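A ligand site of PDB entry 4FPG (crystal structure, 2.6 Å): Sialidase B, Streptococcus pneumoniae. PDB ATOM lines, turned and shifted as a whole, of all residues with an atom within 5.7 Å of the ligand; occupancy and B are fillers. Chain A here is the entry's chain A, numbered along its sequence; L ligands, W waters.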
ATOM      1  N   ARG A 245      17.493  19.828  33.477  1.00  0.00           N
ATOM      2  CA  ARG A 245      16.815  18.622  32.994  1.00  0.00           C
ATOM      3  C   ARG A 245      17.588  17.388  33.418  1.00  0.00           C
ATOM      4  O   ARG A 245      18.797  17.440  33.624  1.00  0.00           O
ATOM      5  CB  ARG A 245      16.673  18.624  31.468  1.00  0.00           C
ATOM      6  CG  ARG A 245      15.341  19.131  30.963  1.00  0.00           C
ATOM      7  CD  ARG A 245      14.856  18.391  29.709  1.00  0.00           C
ATOM      8  NE  ARG A 245      14.546  16.995  29.984  1.00  0.00           N
ATOM      9  CZ  ARG A 245      14.020  16.152  29.102  1.00  0.00           C
ATOM     10  NH1 ARG A 245      13.748  16.556  27.849  1.00  0.00           N
ATOM     11  NH2 ARG A 245      13.779  14.890  29.458  1.00  0.00           N
ATOM     12  N   ILE A 246      16.858  16.282  33.547  1.00  0.00           N
ATOM     13  CA  ILE A 246      17.419  14.980  33.879  1.00  0.00           C
ATOM     14  C   ILE A 246      18.022  14.937  35.304  1.00  0.00           C
ATOM     15  O   ILE A 246      19.241  14.837  35.470  1.00  0.00           O
ATOM     16  CB  ILE A 246      18.456  14.485  32.830  1.00  0.00           C
ATOM     17  CG1 ILE A 246      18.117  14.959  31.415  1.00  0.00           C
ATOM     18  CG2 ILE A 246      18.537  12.988  32.842  1.00  0.00           C
ATOM     19  CD1 ILE A 246      16.752  14.519  30.909  1.00  0.00           C
ATOM     20  N   ARG A 264      21.351  22.878  31.326  1.00  0.00           N
ATOM     21  CA  ARG A 264      21.063  23.165  29.920  1.00  0.00           C
ATOM     22  C   ARG A 264      20.931  24.657  29.621  1.00  0.00           C
ATOM     23  O   ARG A 264      20.036  25.333  30.142  1.00  0.00           O
ATOM     24  CB  ARG A 264      19.822  22.390  29.464  1.00  0.00           C
ATOM     25  CG  ARG A 264      19.990  20.882  29.656  1.00  0.00           C
ATOM     26  CD  ARG A 264      18.863  20.076  29.090  1.00  0.00           C
ATOM     27  NE  ARG A 264      19.302  18.723  28.749  1.00  0.00           N
ATOM     28  CZ  ARG A 264      18.520  17.826  28.142  1.00  0.00           C
ATOM     29  NH1 ARG A 264      17.272  18.139  27.820  1.00  0.00           N
ATOM     30  NH2 ARG A 264      18.994  16.620  27.851  1.00  0.00           N
ATOM     31  N   ASP A 270      18.014  18.642  23.906  1.00  0.00           N
ATOM     32  CA  ASP A 270      19.139  17.709  24.004  1.00  0.00           C
ATOM     33  C   ASP A 270      20.309  18.270  23.168  1.00  0.00           C
ATOM     34  O   ASP A 270      20.152  19.285  22.466  1.00  0.00           O
ATOM     35  CB  ASP A 270      18.770  16.316  23.448  1.00  0.00           C
ATOM     36  CG  ASP A 270      17.641  15.648  24.225  1.00  0.00           C
ATOM     37  OD1 ASP A 270      17.049  14.672  23.708  1.00  0.00           O
ATOM     38  OD2 ASP A 270      17.327  16.094  25.345  1.00  0.00           O
ATOM     39  N   SER A 271      21.466  17.620  23.243  1.00  0.00           N
ATOM     40  CA  SER A 271      22.546  17.902  22.302  1.00  0.00           C
ATOM     41  C   SER A 271      21.973  17.685  20.901  1.00  0.00           C
ATOM     42  O   SER A 271      21.167  16.782  20.708  1.00  0.00           O
ATOM     43  CB  SER A 271      23.729  16.971  22.560  1.00  0.00           C
ATOM     44  OG  SER A 271      24.032  16.865  23.936  1.00  0.00           O
ATOM     45  N   LYS A 272      22.375  18.482  19.904  1.00  0.00           N
ATOM     46  CA  LYS A 272      23.388  19.521  20.053  1.00  0.00           C
ATOM     47  C   LYS A 272      22.877  20.769  20.772  1.00  0.00           C
ATOM     48  O   LYS A 272      21.765  21.242  20.519  1.00  0.00           O
ATOM     49  CB  LYS A 272      23.960  19.892  18.676  1.00  0.00           C
ATOM     50  CG  LYS A 272      22.928  20.450  17.697  1.00  0.00           C
ATOM     51  CD  LYS A 272      23.520  20.679  16.308  1.00  0.00           C
ATOM     52  CE  LYS A 272      22.431  21.058  15.301  1.00  0.00           C
ATOM     53  NZ  LYS A 272      21.788  22.373  15.590  1.00  0.00           N
ATOM     54  N   ILE A 326      25.465  15.155  28.666  1.00  0.00           N
ATOM     55  CA  ILE A 326      24.036  14.859  28.808  1.00  0.00           C
ATOM     56  C   ILE A 326      23.865  13.486  29.416  1.00  0.00           C
ATOM     57  O   ILE A 326      24.673  12.598  29.130  1.00  0.00           O
ATOM     58  CB  ILE A 326      23.324  14.975  27.421  1.00  0.00           C
ATOM     59  CG1 ILE A 326      21.870  14.517  27.496  1.00  0.00           C
ATOM     60  CG2 ILE A 326      24.086  14.219  26.346  1.00  0.00           C
ATOM     61  CD1 ILE A 326      21.115  14.869  26.249  1.00  0.00           C
ATOM     62  N   ASP A 327      22.857  13.308  30.258  1.00  0.00           N
ATOM     63  CA  ASP A 327      22.613  12.026  30.941  1.00  0.00           C
ATOM     64  C   ASP A 327      23.694  11.638  31.996  1.00  0.00           C
ATOM     65  O   ASP A 327      24.564  10.791  31.745  1.00  0.00           O
ATOM     66  CB  ASP A 327      22.441  10.868  29.938  1.00  0.00           C
ATOM     67  CG  ASP A 327      21.186  10.991  29.119  1.00  0.00           C
ATOM     68  OD1 ASP A 327      20.384  11.914  29.399  1.00  0.00           O
ATOM     69  OD2 ASP A 327      20.996  10.161  28.194  1.00  0.00           O
ATOM     70  N   ASP A 344      27.017  11.068  29.324  1.00  0.00           N
ATOM     71  CA  ASP A 344      27.294  11.054  27.894  1.00  0.00           C
ATOM     72  C   ASP A 344      28.056  12.330  27.526  1.00  0.00           C
ATOM     73  O   ASP A 344      27.816  13.396  28.101  1.00  0.00           O
ATOM     74  CB  ASP A 344      26.003  10.917  27.064  1.00  0.00           C
ATOM     75  CG  ASP A 344      25.290   9.593  27.277  1.00  0.00           C
ATOM     76  OD1 ASP A 344      25.968   8.541  27.323  1.00  0.00           O
ATOM     77  OD2 ASP A 344      24.046   9.595  27.398  1.00  0.00           O
ATOM     78  N   MET A 346      29.477  14.781  24.280  1.00  0.00           N
ATOM     79  CA  MET A 346      29.247  15.091  22.866  1.00  0.00           C
ATOM     80  C   MET A 346      30.230  16.148  22.415  1.00  0.00           C
ATOM     81  O   MET A 346      30.411  17.157  23.077  1.00  0.00           O
ATOM     82  CB  MET A 346      27.815  15.598  22.679  1.00  0.00           C
ATOM     83  CG  MET A 346      26.744  14.694  23.276  1.00  0.00           C
ATOM     84  SD  MET A 346      26.046  13.545  22.085  1.00  0.00           S
ATOM     85  CE  MET A 346      25.470  12.252  23.166  1.00  0.00           C
ATOM     86  N   GLY A 351      25.013  15.163  18.650  1.00  0.00           N
ATOM     87  CA  GLY A 351      23.974  14.647  19.518  1.00  0.00           C
ATOM     88  C   GLY A 351      23.420  13.340  19.004  1.00  0.00           C
ATOM     89  O   GLY A 351      23.981  12.747  18.096  1.00  0.00           O
ATOM     90  N   ASN A 352      22.324  12.898  19.616  1.00  0.00           N
ATOM     91  CA  ASN A 352      21.567  11.693  19.240  1.00  0.00           C
ATOM     92  C   ASN A 352      21.443  11.452  17.731  1.00  0.00           C
ATOM     93  O   ASN A 352      21.817  10.397  17.212  1.00  0.00           O
ATOM     94  CB  ASN A 352      20.147  11.788  19.822  1.00  0.00           C
ATOM     95  CG  ASN A 352      19.750  10.564  20.631  1.00  0.00           C
ATOM     96  OD1 ASN A 352      20.525   9.630  20.801  1.00  0.00           O
ATOM     97  ND2 ASN A 352      18.520  10.588  21.146  1.00  0.00           N
ATOM     98  N   ASN A 353      20.922  12.458  17.041  1.00  0.00           N
ATOM     99  CA  ASN A 353      20.505  12.308  15.648  1.00  0.00           C
ATOM    100  C   ASN A 353      21.622  12.317  14.595  1.00  0.00           C
ATOM    101  O   ASN A 353      21.493  11.687  13.538  1.00  0.00           O
ATOM    102  CB  ASN A 353      19.450  13.373  15.307  1.00  0.00           C
ATOM    103  CG  ASN A 353      18.363  13.461  16.361  1.00  0.00           C
ATOM    104  OD1 ASN A 353      18.234  12.567  17.219  1.00  0.00           O
ATOM    105  ND2 ASN A 353      17.563  14.523  16.297  1.00  0.00           N
ATOM    106  N   TYR A 489      24.585   4.372  25.155  1.00  0.00           N
ATOM    107  CA  TYR A 489      24.023   5.557  25.792  1.00  0.00           C
ATOM    108  C   TYR A 489      23.780   5.359  27.297  1.00  0.00           C
ATOM    109  O   TYR A 489      23.035   4.472  27.698  1.00  0.00           O
ATOM    110  CB  TYR A 489      22.719   5.936  25.092  1.00  0.00           C
ATOM    111  CG  TYR A 489      22.954   6.595  23.751  1.00  0.00           C
ATOM    112  CD1 TYR A 489      23.295   7.936  23.676  1.00  0.00           C
ATOM    113  CD2 TYR A 489      22.855   5.862  22.573  1.00  0.00           C
ATOM    114  CE1 TYR A 489      23.539   8.539  22.467  1.00  0.00           C
ATOM    115  CE2 TYR A 489      23.083   6.470  21.362  1.00  0.00           C
ATOM    116  CZ  TYR A 489      23.430   7.809  21.318  1.00  0.00           C
ATOM    117  OH  TYR A 489      23.667   8.430  20.112  1.00  0.00           O
ATOM    118  N   TYR A 509      22.369   1.774  27.239  1.00  0.00           N
ATOM    119  CA  TYR A 509      21.542   1.159  26.201  1.00  0.00           C
ATOM    120  C   TYR A 509      22.046   1.495  24.803  1.00  0.00           C
ATOM    121  O   TYR A 509      22.611   2.564  24.557  1.00  0.00           O
ATOM    122  CB  TYR A 509      20.062   1.574  26.356  1.00  0.00           C
ATOM    123  CG  TYR A 509      19.779   3.025  26.011  1.00  0.00           C
ATOM    124  CD1 TYR A 509      19.351   3.385  24.725  1.00  0.00           C
ATOM    125  CD2 TYR A 509      19.932   4.034  26.944  1.00  0.00           C
ATOM    126  CE1 TYR A 509      19.089   4.692  24.391  1.00  0.00           C
ATOM    127  CE2 TYR A 509      19.671   5.351  26.620  1.00  0.00           C
ATOM    128  CZ  TYR A 509      19.249   5.680  25.343  1.00  0.00           C
ATOM    129  OH  TYR A 509      18.991   6.987  25.018  1.00  0.00           O
ATOM    130  N   THR A 539      14.745   4.312  23.485  1.00  0.00           N
ATOM    131  CA  THR A 539      15.470   5.008  24.512  1.00  0.00           C
ATOM    132  C   THR A 539      15.321   4.137  25.746  1.00  0.00           C
ATOM    133  O   THR A 539      14.536   4.423  26.639  1.00  0.00           O
ATOM    134  CB  THR A 539      14.892   6.420  24.729  1.00  0.00           C
ATOM    135  OG1 THR A 539      14.717   7.036  23.447  1.00  0.00           O
ATOM    136  CG2 THR A 539      15.825   7.249  25.567  1.00  0.00           C
ATOM    137  N   GLU A 541      16.098   3.575  28.626  1.00  0.00           N
ATOM    138  CA  GLU A 541      16.648   4.082  29.875  1.00  0.00           C
ATOM    139  C   GLU A 541      16.276   3.109  30.992  1.00  0.00           C
ATOM    140  O   GLU A 541      15.095   2.870  31.264  1.00  0.00           O
ATOM    141  CB  GLU A 541      16.158   5.511  30.137  1.00  0.00           C
ATOM    142  CG  GLU A 541      16.714   6.509  29.118  1.00  0.00           C
ATOM    143  CD  GLU A 541      15.820   7.725  28.911  1.00  0.00           C
ATOM    144  OE1 GLU A 541      16.354   8.805  28.568  1.00  0.00           O
ATOM    145  OE2 GLU A 541      14.587   7.594  29.103  1.00  0.00           O
ATOM    146  N   ARG A 557      12.455   1.758  30.135  1.00  0.00           N
ATOM    147  CA  ARG A 557      11.548   2.461  29.241  1.00  0.00           C
ATOM    148  C   ARG A 557      11.479   1.748  27.903  1.00  0.00           C
ATOM    149  O   ARG A 557      12.504   1.313  27.392  1.00  0.00           O
ATOM    150  CB  ARG A 557      12.083   3.879  29.043  1.00  0.00           C
ATOM    151  CG  ARG A 557      11.536   4.655  27.856  1.00  0.00           C
ATOM    152  CD  ARG A 557      12.152   6.051  27.821  1.00  0.00           C
ATOM    153  NE  ARG A 557      11.713   6.821  26.671  1.00  0.00           N
ATOM    154  CZ  ARG A 557      12.041   8.089  26.439  1.00  0.00           C
ATOM    155  NH1 ARG A 557      12.832   8.747  27.281  1.00  0.00           N
ATOM    156  NH2 ARG A 557      11.561   8.706  25.363  1.00  0.00           N
ATOM    157  N   GLY A 590       7.484   6.806  25.505  1.00  0.00           N
ATOM    158  CA  GLY A 590       7.852   6.488  26.874  1.00  0.00           C
ATOM    159  C   GLY A 590       8.688   7.541  27.600  1.00  0.00           C
ATOM    160  O   GLY A 590       9.055   8.555  27.020  1.00  0.00           O
ATOM    161  N   ARG A 619       3.319  13.124  29.229  1.00  0.00           N
ATOM    162  CA  ARG A 619       4.124  13.022  30.436  1.00  0.00           C
ATOM    163  C   ARG A 619       3.501  13.821  31.584  1.00  0.00           C
ATOM    164  O   ARG A 619       3.866  14.968  31.856  1.00  0.00           O
ATOM    165  CB  ARG A 619       5.568  13.425  30.156  1.00  0.00           C
ATOM    166  CG  ARG A 619       6.264  12.447  29.206  1.00  0.00           C
ATOM    167  CD  ARG A 619       7.635  12.909  28.837  1.00  0.00           C
ATOM    168  NE  ARG A 619       8.456  11.818  28.312  1.00  0.00           N
ATOM    169  CZ  ARG A 619       9.687  11.994  27.829  1.00  0.00           C
ATOM    170  NH1 ARG A 619      10.228  13.208  27.820  1.00  0.00           N
ATOM    171  NH2 ARG A 619      10.388  10.970  27.359  1.00  0.00           N
ATOM    172  N   TYR A 653      10.934  13.001  33.604  1.00  0.00           N
ATOM    173  CA  TYR A 653      12.123  12.399  34.173  1.00  0.00           C
ATOM    174  C   TYR A 653      12.128  12.638  35.685  1.00  0.00           C
ATOM    175  O   TYR A 653      11.705  13.701  36.161  1.00  0.00           O
ATOM    176  CB  TYR A 653      13.369  12.978  33.523  1.00  0.00           C
ATOM    177  CG  TYR A 653      13.734  12.327  32.212  1.00  0.00           C
ATOM    178  CD1 TYR A 653      12.844  12.316  31.144  1.00  0.00           C
ATOM    179  CD2 TYR A 653      14.976  11.717  32.041  1.00  0.00           C
ATOM    180  CE1 TYR A 653      13.167  11.710  29.952  1.00  0.00           C
ATOM    181  CE2 TYR A 653      15.311  11.118  30.832  1.00  0.00           C
ATOM    182  CZ  TYR A 653      14.402  11.118  29.783  1.00  0.00           C
ATOM    183  OH  TYR A 653      14.717  10.534  28.572  1.00  0.00           O
ATOM    184  N   SER A 673       8.242  17.349  29.370  1.00  0.00           N
ATOM    185  CA  SER A 673       9.495  17.642  28.701  1.00  0.00           C
ATOM    186  C   SER A 673       9.576  17.001  27.318  1.00  0.00           C
ATOM    187  O   SER A 673      10.609  17.050  26.649  1.00  0.00           O
ATOM    188  CB  SER A 673      10.654  17.146  29.558  1.00  0.00           C
ATOM    189  OG  SER A 673      10.485  15.791  29.929  1.00  0.00           O
ATOM    190  N   TRP A 674       8.465  16.388  26.899  1.00  0.00           N
ATOM    191  CA  TRP A 674       8.398  15.849  25.549  1.00  0.00           C
ATOM    192  C   TRP A 674       7.714  16.852  24.638  1.00  0.00           C
ATOM    193  O   TRP A 674       8.146  17.074  23.518  1.00  0.00           O
ATOM    194  CB  TRP A 674       7.667  14.493  25.515  1.00  0.00           C
ATOM    195  CG  TRP A 674       7.598  13.946  24.132  1.00  0.00           C
ATOM    196  CD1 TRP A 674       6.626  14.178  23.201  1.00  0.00           C
ATOM    197  CD2 TRP A 674       8.565  13.085  23.499  1.00  0.00           C
ATOM    198  NE1 TRP A 674       6.917  13.513  22.040  1.00  0.00           N
ATOM    199  CE2 TRP A 674       8.103  12.833  22.191  1.00  0.00           C
ATOM    200  CE3 TRP A 674       9.766  12.496  23.917  1.00  0.00           C
ATOM    201  CZ2 TRP A 674       8.804  12.031  21.305  1.00  0.00           C
ATOM    202  CZ3 TRP A 674      10.450  11.687  23.040  1.00  0.00           C
ATOM    203  CH2 TRP A 674       9.969  11.459  21.739  1.00  0.00           C
HETATM  204  O1  LIG L   1      13.763  13.141  24.308  1.00  0.00           O
HETATM  205  S1  LIG L   1      13.596  12.808  25.751  1.00  0.00           S
HETATM  206  O2  LIG L   1      12.891  11.502  25.925  1.00  0.00           O
HETATM  207  O3  LIG L   1      12.788  13.892  26.459  1.00  0.00           O
HETATM  208  C1  LIG L   1      15.226  12.696  26.396  1.00  0.00           C
HETATM  209  C2  LIG L   1      16.202  11.908  25.541  1.00  0.00           C
HETATM  210  N1  LIG L   1      17.618  12.079  25.849  1.00  0.00           N
HETATM  211  C3  LIG L   1      18.394  11.148  25.024  1.00  0.00           C
HETATM  212  C4  LIG L   1      19.718  11.680  24.461  1.00  0.00           C
HETATM  213  C5  LIG L   1      19.697  12.664  23.459  1.00  0.00           C
HETATM  214  C6  LIG L   1      20.907  11.197  24.945  1.00  0.00           C
HETATM  215  C7  LIG L   1      22.166  11.713  24.404  1.00  0.00           C
HETATM  216  C8  LIG L   1      22.136  12.668  23.431  1.00  0.00           C
HETATM  217  C9  LIG L   1      20.919  13.174  22.937  1.00  0.00           C
HETATM  218  O4  LIG L   1      20.918  14.144  21.937  1.00  0.00           O
HETATM  219  O   HOH W   1      18.656   8.942  27.459  1.00  0.00           O
HETATM  220  O   HOH W   2      13.236  16.096  23.575  1.00  0.00           O
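The backbone carbonyl oxygen (O) of Ser 271 lies within hydrogen-bond range of an oxygen (O4) of the ligand (2.9 Å).
The guanidinium group (NH2) of Arg 619 is in salt-bridge range of an oxygen (O2) of the ligand (2.9 Å).
The backbone NH of Asn 352 is in hydrogen-bond range of an oxygen (O4) of the ligand (3.0 Å).
An oxygen (O2) of the ligand lies within salt-bridge range of the guanidinium group of Arg 557 (3.1 Å).
OH of Tyr 653 lies close to O2 of the ligand, at 3.4 Å.
The guanidinium group (NH1) of Arg 245 is in salt-bridge range of an oxygen (O3) of the ligand, at 3.2 Å.
The side-chain carboxylate of Asp 270 is in salt-bridge range of a nitrogen (N1) of the ligand, at 3.4 Å.
The guanidinium group of Arg 619 sits at hydrogen-bond distance from the side-chain hydroxyl of Ser 673 (3.3 Å).
The backbone carbonyl oxygen (O) of Gly 590 lies within hydrogen-bond range of the guanidinium group (NH2) of Arg 619, at 2.8 Å.
The side-chain hydroxyl of Tyr 653 sits at hydrogen-bond distance from the guanidinium group of Arg 557 (2.9 Å).
NH1 of Arg 557 lies within salt-bridge range of OE2 of Glu 541, at 2.8 Å.
OE2 of Glu 541 lies within hydrogen-bond range of OH of Tyr 653.
NH1 of Arg 245 is in hydrogen-bond range of O of Ser 673.
The side-chain carboxylate (OD2) of Asp 270 lies within salt-bridge range of the guanidinium group (NH2) of Arg 264.
The backbone carbonyl oxygen (O) of Asp 327 lies within hydrogen-bond range of the backbone NH (N) of Asp 344 (3.5 Å).
Merely in contact with the ligand: Met 346 (3.4 Å), Asp 327 (3.4 Å), Ile 326 (3.7 Å), Trp 674 (3.8 Å), Ser 673 (3.8 Å), Gly 351 (3.9 Å) and Tyr 489 (3.96 Å).
Hydrophobic or aromatic side chains within 4 Å of the ligand: Ile 326, Met 346, Tyr 489, Tyr 653 and Trp 674.
14 residues have an atom within 4 Å of the ligand: Arg 245, Asp 270, Ser 271, Ile 326, Asp 327, Met 346, Gly 351, Asn 352, Tyr 489, Arg 557, Arg 619, Tyr 653, Ser 673 and Trp 674.
The nearest printed residue that does not touch the ligand is Asp 344 (4.1 Å).
Water W1 lies within hydrogen-bond range of the side-chain carboxylate (OE1) of Glu 541 (2.6 Å), the side-chain carboxylate (OD2) of Asp 327 (2.7 Å) and the side-chain hydroxyl (OH) of Tyr 509 (3.1 Å).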
